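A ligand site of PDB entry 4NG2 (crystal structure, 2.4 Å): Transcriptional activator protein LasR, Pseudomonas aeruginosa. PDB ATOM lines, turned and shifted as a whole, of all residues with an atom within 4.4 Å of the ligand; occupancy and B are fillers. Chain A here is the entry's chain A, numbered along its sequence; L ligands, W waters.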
ATOM      1  N   LEU A  50       6.051 -21.542   4.059  1.00  0.00           N
ATOM      2  CA  LEU A  50       6.485 -22.661   3.234  1.00  0.00           C
ATOM      3  C   LEU A  50       6.559 -22.204   1.765  1.00  0.00           C
ATOM      4  O   LEU A  50       5.700 -21.447   1.283  1.00  0.00           O
ATOM      5  CB  LEU A  50       5.539 -23.853   3.389  1.00  0.00           C
ATOM      6  CG  LEU A  50       5.920 -25.186   2.722  1.00  0.00           C
ATOM      7  CD1 LEU A  50       5.227 -26.365   3.375  1.00  0.00           C
ATOM      8  CD2 LEU A  50       5.643 -25.191   1.206  1.00  0.00           C
ATOM      9  N   GLY A  52       7.233 -24.011  -2.021  1.00  0.00           N
ATOM     10  CA  GLY A  52       7.326 -25.274  -2.735  1.00  0.00           C
ATOM     11  C   GLY A  52       7.380 -25.040  -4.227  1.00  0.00           C
ATOM     12  O   GLY A  52       6.636 -24.199  -4.734  1.00  0.00           O
ATOM     13  N   LEU A  53       8.241 -25.763  -4.935  1.00  0.00           N
ATOM     14  CA  LEU A  53       8.432 -25.484  -6.354  1.00  0.00           C
ATOM     15  C   LEU A  53       8.852 -26.739  -7.129  1.00  0.00           C
ATOM     16  O   LEU A  53       9.862 -27.374  -6.814  1.00  0.00           O
ATOM     17  CB  LEU A  53       9.492 -24.379  -6.531  1.00  0.00           C
ATOM     18  CG  LEU A  53       9.740 -23.754  -7.912  1.00  0.00           C
ATOM     19  CD1 LEU A  53       8.519 -22.930  -8.401  1.00  0.00           C
ATOM     20  CD2 LEU A  53      11.020 -22.885  -7.881  1.00  0.00           C
ATOM     21  N   LEU A  54       8.054 -27.093  -8.131  1.00  0.00           N
ATOM     22  CA  LEU A  54       8.373 -28.199  -9.025  1.00  0.00           C
ATOM     23  C   LEU A  54       8.889 -27.684 -10.366  1.00  0.00           C
ATOM     24  O   LEU A  54       8.607 -26.542 -10.762  1.00  0.00           O
ATOM     25  CB  LEU A  54       7.125 -29.066  -9.249  1.00  0.00           C
ATOM     26  CG  LEU A  54       6.681 -29.862  -8.023  1.00  0.00           C
ATOM     27  CD1 LEU A  54       5.172 -30.133  -8.047  1.00  0.00           C
ATOM     28  CD2 LEU A  54       7.470 -31.160  -7.960  1.00  0.00           C
ATOM     29  N   TYR A  61       4.750 -33.944  -6.076  1.00  0.00           N
ATOM     30  CA  TYR A  61       4.656 -33.019  -4.944  1.00  0.00           C
ATOM     31  C   TYR A  61       5.665 -33.268  -3.806  1.00  0.00           C
ATOM     32  O   TYR A  61       6.363 -32.346  -3.338  1.00  0.00           O
ATOM     33  CB  TYR A  61       3.226 -33.005  -4.405  1.00  0.00           C
ATOM     34  CG  TYR A  61       2.153 -32.564  -5.410  1.00  0.00           C
ATOM     35  CD1 TYR A  61       2.377 -31.490  -6.268  1.00  0.00           C
ATOM     36  CD2 TYR A  61       0.931 -33.219  -5.489  1.00  0.00           C
ATOM     37  CE1 TYR A  61       1.399 -31.092  -7.176  1.00  0.00           C
ATOM     38  CE2 TYR A  61      -0.050 -32.829  -6.403  1.00  0.00           C
ATOM     39  CZ  TYR A  61       0.190 -31.760  -7.246  1.00  0.00           C
ATOM     40  OH  TYR A  61      -0.778 -31.371  -8.133  1.00  0.00           O
ATOM     41  N   ALA A  64       9.352 -32.167  -4.588  1.00  0.00           N
ATOM     42  CA  ALA A  64       9.646 -30.806  -5.011  1.00  0.00           C
ATOM     43  C   ALA A  64      10.697 -30.198  -4.106  1.00  0.00           C
ATOM     44  O   ALA A  64      10.996 -30.736  -3.034  1.00  0.00           O
ATOM     45  CB  ALA A  64       8.385 -29.952  -4.955  1.00  0.00           C
ATOM     46  N   TYR A  70       7.481 -24.885   8.595  1.00  0.00           N
ATOM     47  CA  TYR A  70       6.191 -25.465   8.959  1.00  0.00           C
ATOM     48  C   TYR A  70       6.474 -26.429  10.094  1.00  0.00           C
ATOM     49  O   TYR A  70       7.607 -26.914  10.208  1.00  0.00           O
ATOM     50  CB  TYR A  70       5.537 -26.175   7.780  1.00  0.00           C
ATOM     51  CG  TYR A  70       4.512 -25.318   7.059  1.00  0.00           C
ATOM     52  CD1 TYR A  70       4.358 -23.977   7.379  1.00  0.00           C
ATOM     53  CD2 TYR A  70       3.705 -25.845   6.067  1.00  0.00           C
ATOM     54  CE1 TYR A  70       3.440 -23.186   6.728  1.00  0.00           C
ATOM     55  CE2 TYR A  70       2.771 -25.057   5.411  1.00  0.00           C
ATOM     56  CZ  TYR A  70       2.646 -23.726   5.744  1.00  0.00           C
ATOM     57  OH  TYR A  70       1.728 -22.914   5.101  1.00  0.00           O
ATOM     58  N   TRP A  74       3.830 -31.952  11.342  1.00  0.00           N
ATOM     59  CA  TRP A  74       2.861 -31.771  10.278  1.00  0.00           C
ATOM     60  C   TRP A  74       3.463 -32.031   8.901  1.00  0.00           C
ATOM     61  O   TRP A  74       2.841 -32.651   8.034  1.00  0.00           O
ATOM     62  CB  TRP A  74       2.248 -30.364  10.353  1.00  0.00           C
ATOM     63  CG  TRP A  74       1.446 -29.965   9.148  1.00  0.00           C
ATOM     64  CD1 TRP A  74       1.820 -29.099   8.165  1.00  0.00           C
ATOM     65  CD2 TRP A  74       0.122 -30.405   8.811  1.00  0.00           C
ATOM     66  NE1 TRP A  74       0.815 -28.977   7.235  1.00  0.00           N
ATOM     67  CE2 TRP A  74      -0.230 -29.777   7.600  1.00  0.00           C
ATOM     68  CE3 TRP A  74      -0.789 -31.282   9.405  1.00  0.00           C
ATOM     69  CZ2 TRP A  74      -1.457 -29.993   6.974  1.00  0.00           C
ATOM     70  CZ3 TRP A  74      -2.013 -31.492   8.785  1.00  0.00           C
ATOM     71  CH2 TRP A  74      -2.332 -30.856   7.582  1.00  0.00           C
ATOM     72  N   ARG A  75       4.689 -31.582   8.701  1.00  0.00           N
ATOM     73  CA  ARG A  75       5.321 -31.798   7.419  1.00  0.00           C
ATOM     74  C   ARG A  75       5.467 -33.300   7.174  1.00  0.00           C
ATOM     75  O   ARG A  75       5.135 -33.799   6.089  1.00  0.00           O
ATOM     76  CB  ARG A  75       6.652 -31.058   7.315  1.00  0.00           C
ATOM     77  CG  ARG A  75       6.523 -29.524   7.243  1.00  0.00           C
ATOM     78  CD  ARG A  75       5.940 -29.080   5.909  1.00  0.00           C
ATOM     79  NE  ARG A  75       6.637 -29.779   4.841  1.00  0.00           N
ATOM     80  CZ  ARG A  75       6.039 -30.350   3.794  1.00  0.00           C
ATOM     81  NH1 ARG A  75       4.730 -30.273   3.658  1.00  0.00           N
ATOM     82  NH2 ARG A  75       6.762 -30.979   2.889  1.00  0.00           N
ATOM     83  N   TYR A  78       2.062 -34.639   6.267  1.00  0.00           N
ATOM     84  CA  TYR A  78       1.693 -34.139   4.954  1.00  0.00           C
ATOM     85  C   TYR A  78       2.301 -34.973   3.813  1.00  0.00           C
ATOM     86  O   TYR A  78       1.616 -35.250   2.826  1.00  0.00           O
ATOM     87  CB  TYR A  78       2.146 -32.676   4.832  1.00  0.00           C
ATOM     88  CG  TYR A  78       1.482 -31.857   3.750  1.00  0.00           C
ATOM     89  CD1 TYR A  78       1.924 -31.901   2.429  1.00  0.00           C
ATOM     90  CD2 TYR A  78       0.442 -30.976   4.063  1.00  0.00           C
ATOM     91  CE1 TYR A  78       1.323 -31.112   1.446  1.00  0.00           C
ATOM     92  CE2 TYR A  78      -0.166 -30.189   3.087  1.00  0.00           C
ATOM     93  CZ  TYR A  78       0.277 -30.265   1.786  1.00  0.00           C
ATOM     94  OH  TYR A  78      -0.328 -29.490   0.837  1.00  0.00           O
ATOM     95  N   ASP A  87      -4.989 -30.925  -0.389  1.00  0.00           N
ATOM     96  CA  ASP A  87      -4.886 -29.502  -0.051  1.00  0.00           C
ATOM     97  C   ASP A  87      -5.526 -28.615  -1.110  1.00  0.00           C
ATOM     98  O   ASP A  87      -5.085 -28.591  -2.252  1.00  0.00           O
ATOM     99  CB  ASP A  87      -3.415 -29.116   0.116  1.00  0.00           C
ATOM    100  CG  ASP A  87      -3.238 -27.824   0.886  1.00  0.00           C
ATOM    101  OD1 ASP A  87      -4.181 -27.002   0.930  1.00  0.00           O
ATOM    102  OD2 ASP A  87      -2.138 -27.622   1.447  1.00  0.00           O
ATOM    103  N   THR A  89      -5.346 -25.425  -1.436  1.00  0.00           N
ATOM    104  CA  THR A  89      -4.348 -24.470  -1.922  1.00  0.00           C
ATOM    105  C   THR A  89      -3.447 -25.056  -3.014  1.00  0.00           C
ATOM    106  O   THR A  89      -2.967 -24.326  -3.912  1.00  0.00           O
ATOM    107  CB  THR A  89      -3.420 -24.063  -0.822  1.00  0.00           C
ATOM    108  OG1 THR A  89      -2.517 -25.147  -0.580  1.00  0.00           O
ATOM    109  CG2 THR A  89      -4.207 -23.719   0.441  1.00  0.00           C
ATOM    110  N   VAL A  90      -3.172 -26.355  -2.948  1.00  0.00           N
ATOM    111  CA  VAL A  90      -2.261 -26.926  -3.934  1.00  0.00           C
ATOM    112  C   VAL A  90      -2.902 -26.990  -5.313  1.00  0.00           C
ATOM    113  O   VAL A  90      -2.271 -26.619  -6.307  1.00  0.00           O
ATOM    114  CB  VAL A  90      -1.731 -28.290  -3.521  1.00  0.00           C
ATOM    115  CG1 VAL A  90      -0.849 -28.857  -4.625  1.00  0.00           C
ATOM    116  CG2 VAL A  90      -0.960 -28.190  -2.215  1.00  0.00           C
ATOM    117  N   CYS A  93      -3.247 -23.458  -6.758  1.00  0.00           N
ATOM    118  CA  CYS A  93      -2.007 -23.006  -7.366  1.00  0.00           C
ATOM    119  C   CYS A  93      -1.828 -23.524  -8.797  1.00  0.00           C
ATOM    120  O   CYS A  93      -1.271 -22.811  -9.650  1.00  0.00           O
ATOM    121  CB  CYS A  93      -0.777 -23.403  -6.538  1.00  0.00           C
ATOM    122  SG  CYS A  93      -0.624 -22.581  -4.933  1.00  0.00           S
ATOM    123  N   TRP A 102      -6.959 -18.473   3.291  1.00  0.00           N
ATOM    124  CA  TRP A 102      -7.448 -19.689   3.932  1.00  0.00           C
ATOM    125  C   TRP A 102      -8.804 -19.433   4.636  1.00  0.00           C
ATOM    126  O   TRP A 102      -8.871 -19.430   5.864  1.00  0.00           O
ATOM    127  CB  TRP A 102      -6.409 -20.217   4.926  1.00  0.00           C
ATOM    128  CG  TRP A 102      -5.064 -20.541   4.303  1.00  0.00           C
ATOM    129  CD1 TRP A 102      -4.763 -20.594   2.968  1.00  0.00           C
ATOM    130  CD2 TRP A 102      -3.851 -20.884   4.998  1.00  0.00           C
ATOM    131  NE1 TRP A 102      -3.444 -20.936   2.794  1.00  0.00           N
ATOM    132  CE2 TRP A 102      -2.861 -21.111   4.013  1.00  0.00           C
ATOM    133  CE3 TRP A 102      -3.511 -20.999   6.350  1.00  0.00           C
ATOM    134  CZ2 TRP A 102      -1.543 -21.453   4.351  1.00  0.00           C
ATOM    135  CZ3 TRP A 102      -2.203 -21.342   6.678  1.00  0.00           C
ATOM    136  CH2 TRP A 102      -1.236 -21.567   5.684  1.00  0.00           C
ATOM    137  N   TYR A 107     -12.412 -25.090   1.840  1.00  0.00           N
ATOM    138  CA  TYR A 107     -12.421 -26.491   2.213  1.00  0.00           C
ATOM    139  C   TYR A 107     -13.848 -27.030   2.104  1.00  0.00           C
ATOM    140  O   TYR A 107     -14.649 -26.847   3.014  1.00  0.00           O
ATOM    141  CB  TYR A 107     -11.961 -26.644   3.660  1.00  0.00           C
ATOM    142  CG  TYR A 107     -10.559 -26.113   3.966  1.00  0.00           C
ATOM    143  CD1 TYR A 107      -9.434 -26.735   3.442  1.00  0.00           C
ATOM    144  CD2 TYR A 107     -10.373 -25.030   4.809  1.00  0.00           C
ATOM    145  CE1 TYR A 107      -8.152 -26.274   3.729  1.00  0.00           C
ATOM    146  CE2 TYR A 107      -9.107 -24.552   5.101  1.00  0.00           C
ATOM    147  CZ  TYR A 107      -7.988 -25.188   4.564  1.00  0.00           C
ATOM    148  OH  TYR A 107      -6.719 -24.733   4.865  1.00  0.00           O
ATOM    149  N   PHE A 115      -8.869 -32.433   6.210  1.00  0.00           N
ATOM    150  CA  PHE A 115      -7.555 -31.818   6.082  1.00  0.00           C
ATOM    151  C   PHE A 115      -7.495 -30.555   6.942  1.00  0.00           C
ATOM    152  O   PHE A 115      -6.462 -30.223   7.517  1.00  0.00           O
ATOM    153  CB  PHE A 115      -7.272 -31.494   4.612  1.00  0.00           C
ATOM    154  CG  PHE A 115      -6.035 -30.662   4.387  1.00  0.00           C
ATOM    155  CD1 PHE A 115      -6.082 -29.276   4.537  1.00  0.00           C
ATOM    156  CD2 PHE A 115      -4.836 -31.252   4.013  1.00  0.00           C
ATOM    157  CE1 PHE A 115      -4.963 -28.504   4.329  1.00  0.00           C
ATOM    158  CE2 PHE A 115      -3.704 -30.484   3.802  1.00  0.00           C
ATOM    159  CZ  PHE A 115      -3.761 -29.108   3.953  1.00  0.00           C
ATOM    160  N   ALA A 119      -4.876 -29.495  10.032  1.00  0.00           N
ATOM    161  CA  ALA A 119      -4.065 -28.323   9.742  1.00  0.00           C
ATOM    162  C   ALA A 119      -4.293 -27.292  10.836  1.00  0.00           C
ATOM    163  O   ALA A 119      -3.363 -26.580  11.220  1.00  0.00           O
ATOM    164  CB  ALA A 119      -4.401 -27.726   8.383  1.00  0.00           C
ATOM    165  N   LEU A 124      -1.825 -23.972  11.597  1.00  0.00           N
ATOM    166  CA  LEU A 124      -1.983 -23.404  10.278  1.00  0.00           C
ATOM    167  C   LEU A 124      -3.427 -23.002  10.014  1.00  0.00           C
ATOM    168  O   LEU A 124      -4.055 -23.477   9.065  1.00  0.00           O
ATOM    169  CB  LEU A 124      -1.514 -24.436   9.240  1.00  0.00           C
ATOM    170  CG  LEU A 124      -0.037 -24.787   9.365  1.00  0.00           C
ATOM    171  CD1 LEU A 124       0.223 -26.246   9.031  1.00  0.00           C
ATOM    172  CD2 LEU A 124       0.836 -23.870   8.505  1.00  0.00           C
ATOM    173  N   LEU A 139       6.268 -24.467 -11.528  1.00  0.00           N
ATOM    174  CA  LEU A 139       5.042 -24.399 -10.737  1.00  0.00           C
ATOM    175  C   LEU A 139       5.319 -24.588  -9.255  1.00  0.00           C
ATOM    176  O   LEU A 139       6.077 -25.458  -8.865  1.00  0.00           O
ATOM    177  CB  LEU A 139       4.077 -25.512 -11.158  1.00  0.00           C
ATOM    178  CG  LEU A 139       2.835 -25.647 -10.271  1.00  0.00           C
ATOM    179  CD1 LEU A 139       1.837 -24.552 -10.638  1.00  0.00           C
ATOM    180  CD2 LEU A 139       2.185 -27.020 -10.377  1.00  0.00           C
ATOM    181  N   GLY A 140       4.659 -23.793  -8.411  1.00  0.00           N
ATOM    182  CA  GLY A 140       4.877 -23.891  -6.985  1.00  0.00           C
ATOM    183  C   GLY A 140       3.930 -23.086  -6.137  1.00  0.00           C
ATOM    184  O   GLY A 140       2.946 -22.545  -6.614  1.00  0.00           O
ATOM    185  N   ALA A 141       4.240 -23.002  -4.839  1.00  0.00           N
ATOM    186  CA  ALA A 141       3.355 -22.337  -3.893  1.00  0.00           C
ATOM    187  C   ALA A 141       4.182 -21.675  -2.794  1.00  0.00           C
ATOM    188  O   ALA A 141       5.156 -22.256  -2.313  1.00  0.00           O
ATOM    189  CB  ALA A 141       2.388 -23.349  -3.278  1.00  0.00           C
ATOM    190  N   SER A 143       3.432 -20.038   0.872  1.00  0.00           N
ATOM    191  CA  SER A 143       2.378 -19.906   1.856  1.00  0.00           C
ATOM    192  C   SER A 143       2.909 -19.221   3.093  1.00  0.00           C
ATOM    193  O   SER A 143       4.045 -19.446   3.485  1.00  0.00           O
ATOM    194  CB  SER A 143       1.820 -21.284   2.206  1.00  0.00           C
ATOM    195  OG  SER A 143       1.154 -21.860   1.086  1.00  0.00           O
HETATM  196  C1  LIG L   1       1.953 -26.519  -6.216  1.00  0.00           C
HETATM  197  C2  LIG L   1       2.537 -27.378  -5.145  1.00  0.00           C
HETATM  198  C3  LIG L   1       3.804 -27.991  -5.637  1.00  0.00           C
HETATM  199  C4  LIG L   1       4.807 -28.085  -4.515  1.00  0.00           C
HETATM  200  C5  LIG L   1       4.285 -28.977  -3.412  1.00  0.00           C
HETATM  201  C6  LIG L   1       4.085 -28.160  -2.136  1.00  0.00           C
HETATM  202  C7  LIG L   1       3.462 -29.063  -1.113  1.00  0.00           C
HETATM  203  C8  LIG L   1       3.139 -28.273   0.144  1.00  0.00           C
HETATM  204  C9  LIG L   1       2.048 -27.274  -0.180  1.00  0.00           C
HETATM  205  C10 LIG L   1       1.558 -26.665   1.128  1.00  0.00           C
HETATM  206  O1  LIG L   1       2.127 -26.893   2.189  1.00  0.00           O
HETATM  207  C11 LIG L   1       0.620 -25.480   1.027  1.00  0.00           C
HETATM  208  C12 LIG L   1       0.113 -25.104   2.385  1.00  0.00           C
HETATM  209  O2  LIG L   1       0.593 -24.137   2.975  1.00  0.00           O
HETATM  210  N1  LIG L   1      -1.124 -25.706   2.827  1.00  0.00           N
HETATM  211  C13 LIG L   1      -1.779 -25.167   3.993  1.00  0.00           C
HETATM  212  C14 LIG L   1      -3.256 -25.040   3.836  1.00  0.00           C
HETATM  213  C15 LIG L   1      -3.750 -25.222   5.249  1.00  0.00           C
HETATM  214  C16 LIG L   1      -1.689 -26.096   5.120  1.00  0.00           C
HETATM  215  O3  LIG L   1      -0.705 -26.756   5.413  1.00  0.00           O
HETATM  216  O4  LIG L   1      -2.632 -25.618   5.988  1.00  0.00           O
HETATM  217  O   HOH W   1       2.743 -28.797   4.612  1.00  0.00           O
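The side-chain carboxylate (OD2) of Asp 87 sits at hydrogen-bond distance from a nitrogen (N1) of the ligand, 2.6 Å away.
An oxygen (O2) of the ligand is in hydrogen-bond range of the side-chain hydroxyl (OH) of Tyr 70 (2.7 Å).
The side-chain hydroxyl of Ser 143 sits at hydrogen-bond distance from an oxygen (O2) of the ligand, at 3.0 Å.
O3 of the ligand is in hydrogen-bond range of NE1 of Trp 74.
The side-chain hydroxyl (OH) of Tyr 78 lies within hydrogen-bond range of the side-chain carboxylate (OD2) of Asp 87 (2.7 Å).
OD1 of Asp 87 is in hydrogen-bond range of OG1 of Thr 89 (2.9 Å).
N of Ser 143 is in hydrogen-bond range of O of Leu 50.
N of Leu 54 is in hydrogen-bond range of O of Leu 139, 2.7 Å away.
The backbone carbonyl oxygen (O) of Thr 89 is in hydrogen-bond range of the side-chain sulfur (SG) of Cys 93 (3.1 Å).
The backbone carbonyl oxygen of Ala 119 sits at hydrogen-bond distance from the backbone NH of Leu 124, 3.1 Å away.
The backbone carbonyl oxygen of Gly 52 lies within hydrogen-bond range of the backbone NH of Ala 141 (2.7 Å).
Leu 50 touches the ligand (CD1 to O1, 3.4 Å).
C of Gly 52 touches C4 of the ligand, 3.997 Å away.
Leu 54 touches the ligand (CD1 to C3, 3.5 Å).
Tyr 61 touches the ligand (CD1 to C3, 3.8 Å).
Tyr 78 touches the ligand (OH to C9, 3.4 Å).
Thr 89 touches the ligand.
CG1 of Val 90 touches C2 of the ligand, 3.7 Å away.
Trp 102 touches the ligand.
OH of Tyr 107 touches C15 of the ligand, at 3.0 Å.
CE1 of Phe 115 touches C15 of the ligand (3.6 Å).
Ala 119 touches the ligand (CB to O4, 3.6 Å).
Leu 124 touches the ligand (CB to O4, 3.6 Å).
Gly 140 touches the ligand.
Within 4 Å of the ligand: Leu 50, Gly 52, Leu 54, Tyr 61, Tyr 70, Trp 74, Tyr 78, Asp 87, Thr 89, Val 90, Trp 102, Tyr 107, Phe 115, Ala 119, Leu 124, Gly 140 and Ser 143.
Water W1 lies within hydrogen-bond range of NH1 of Arg 75, O1 of the ligand and NE1 of Trp 74.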
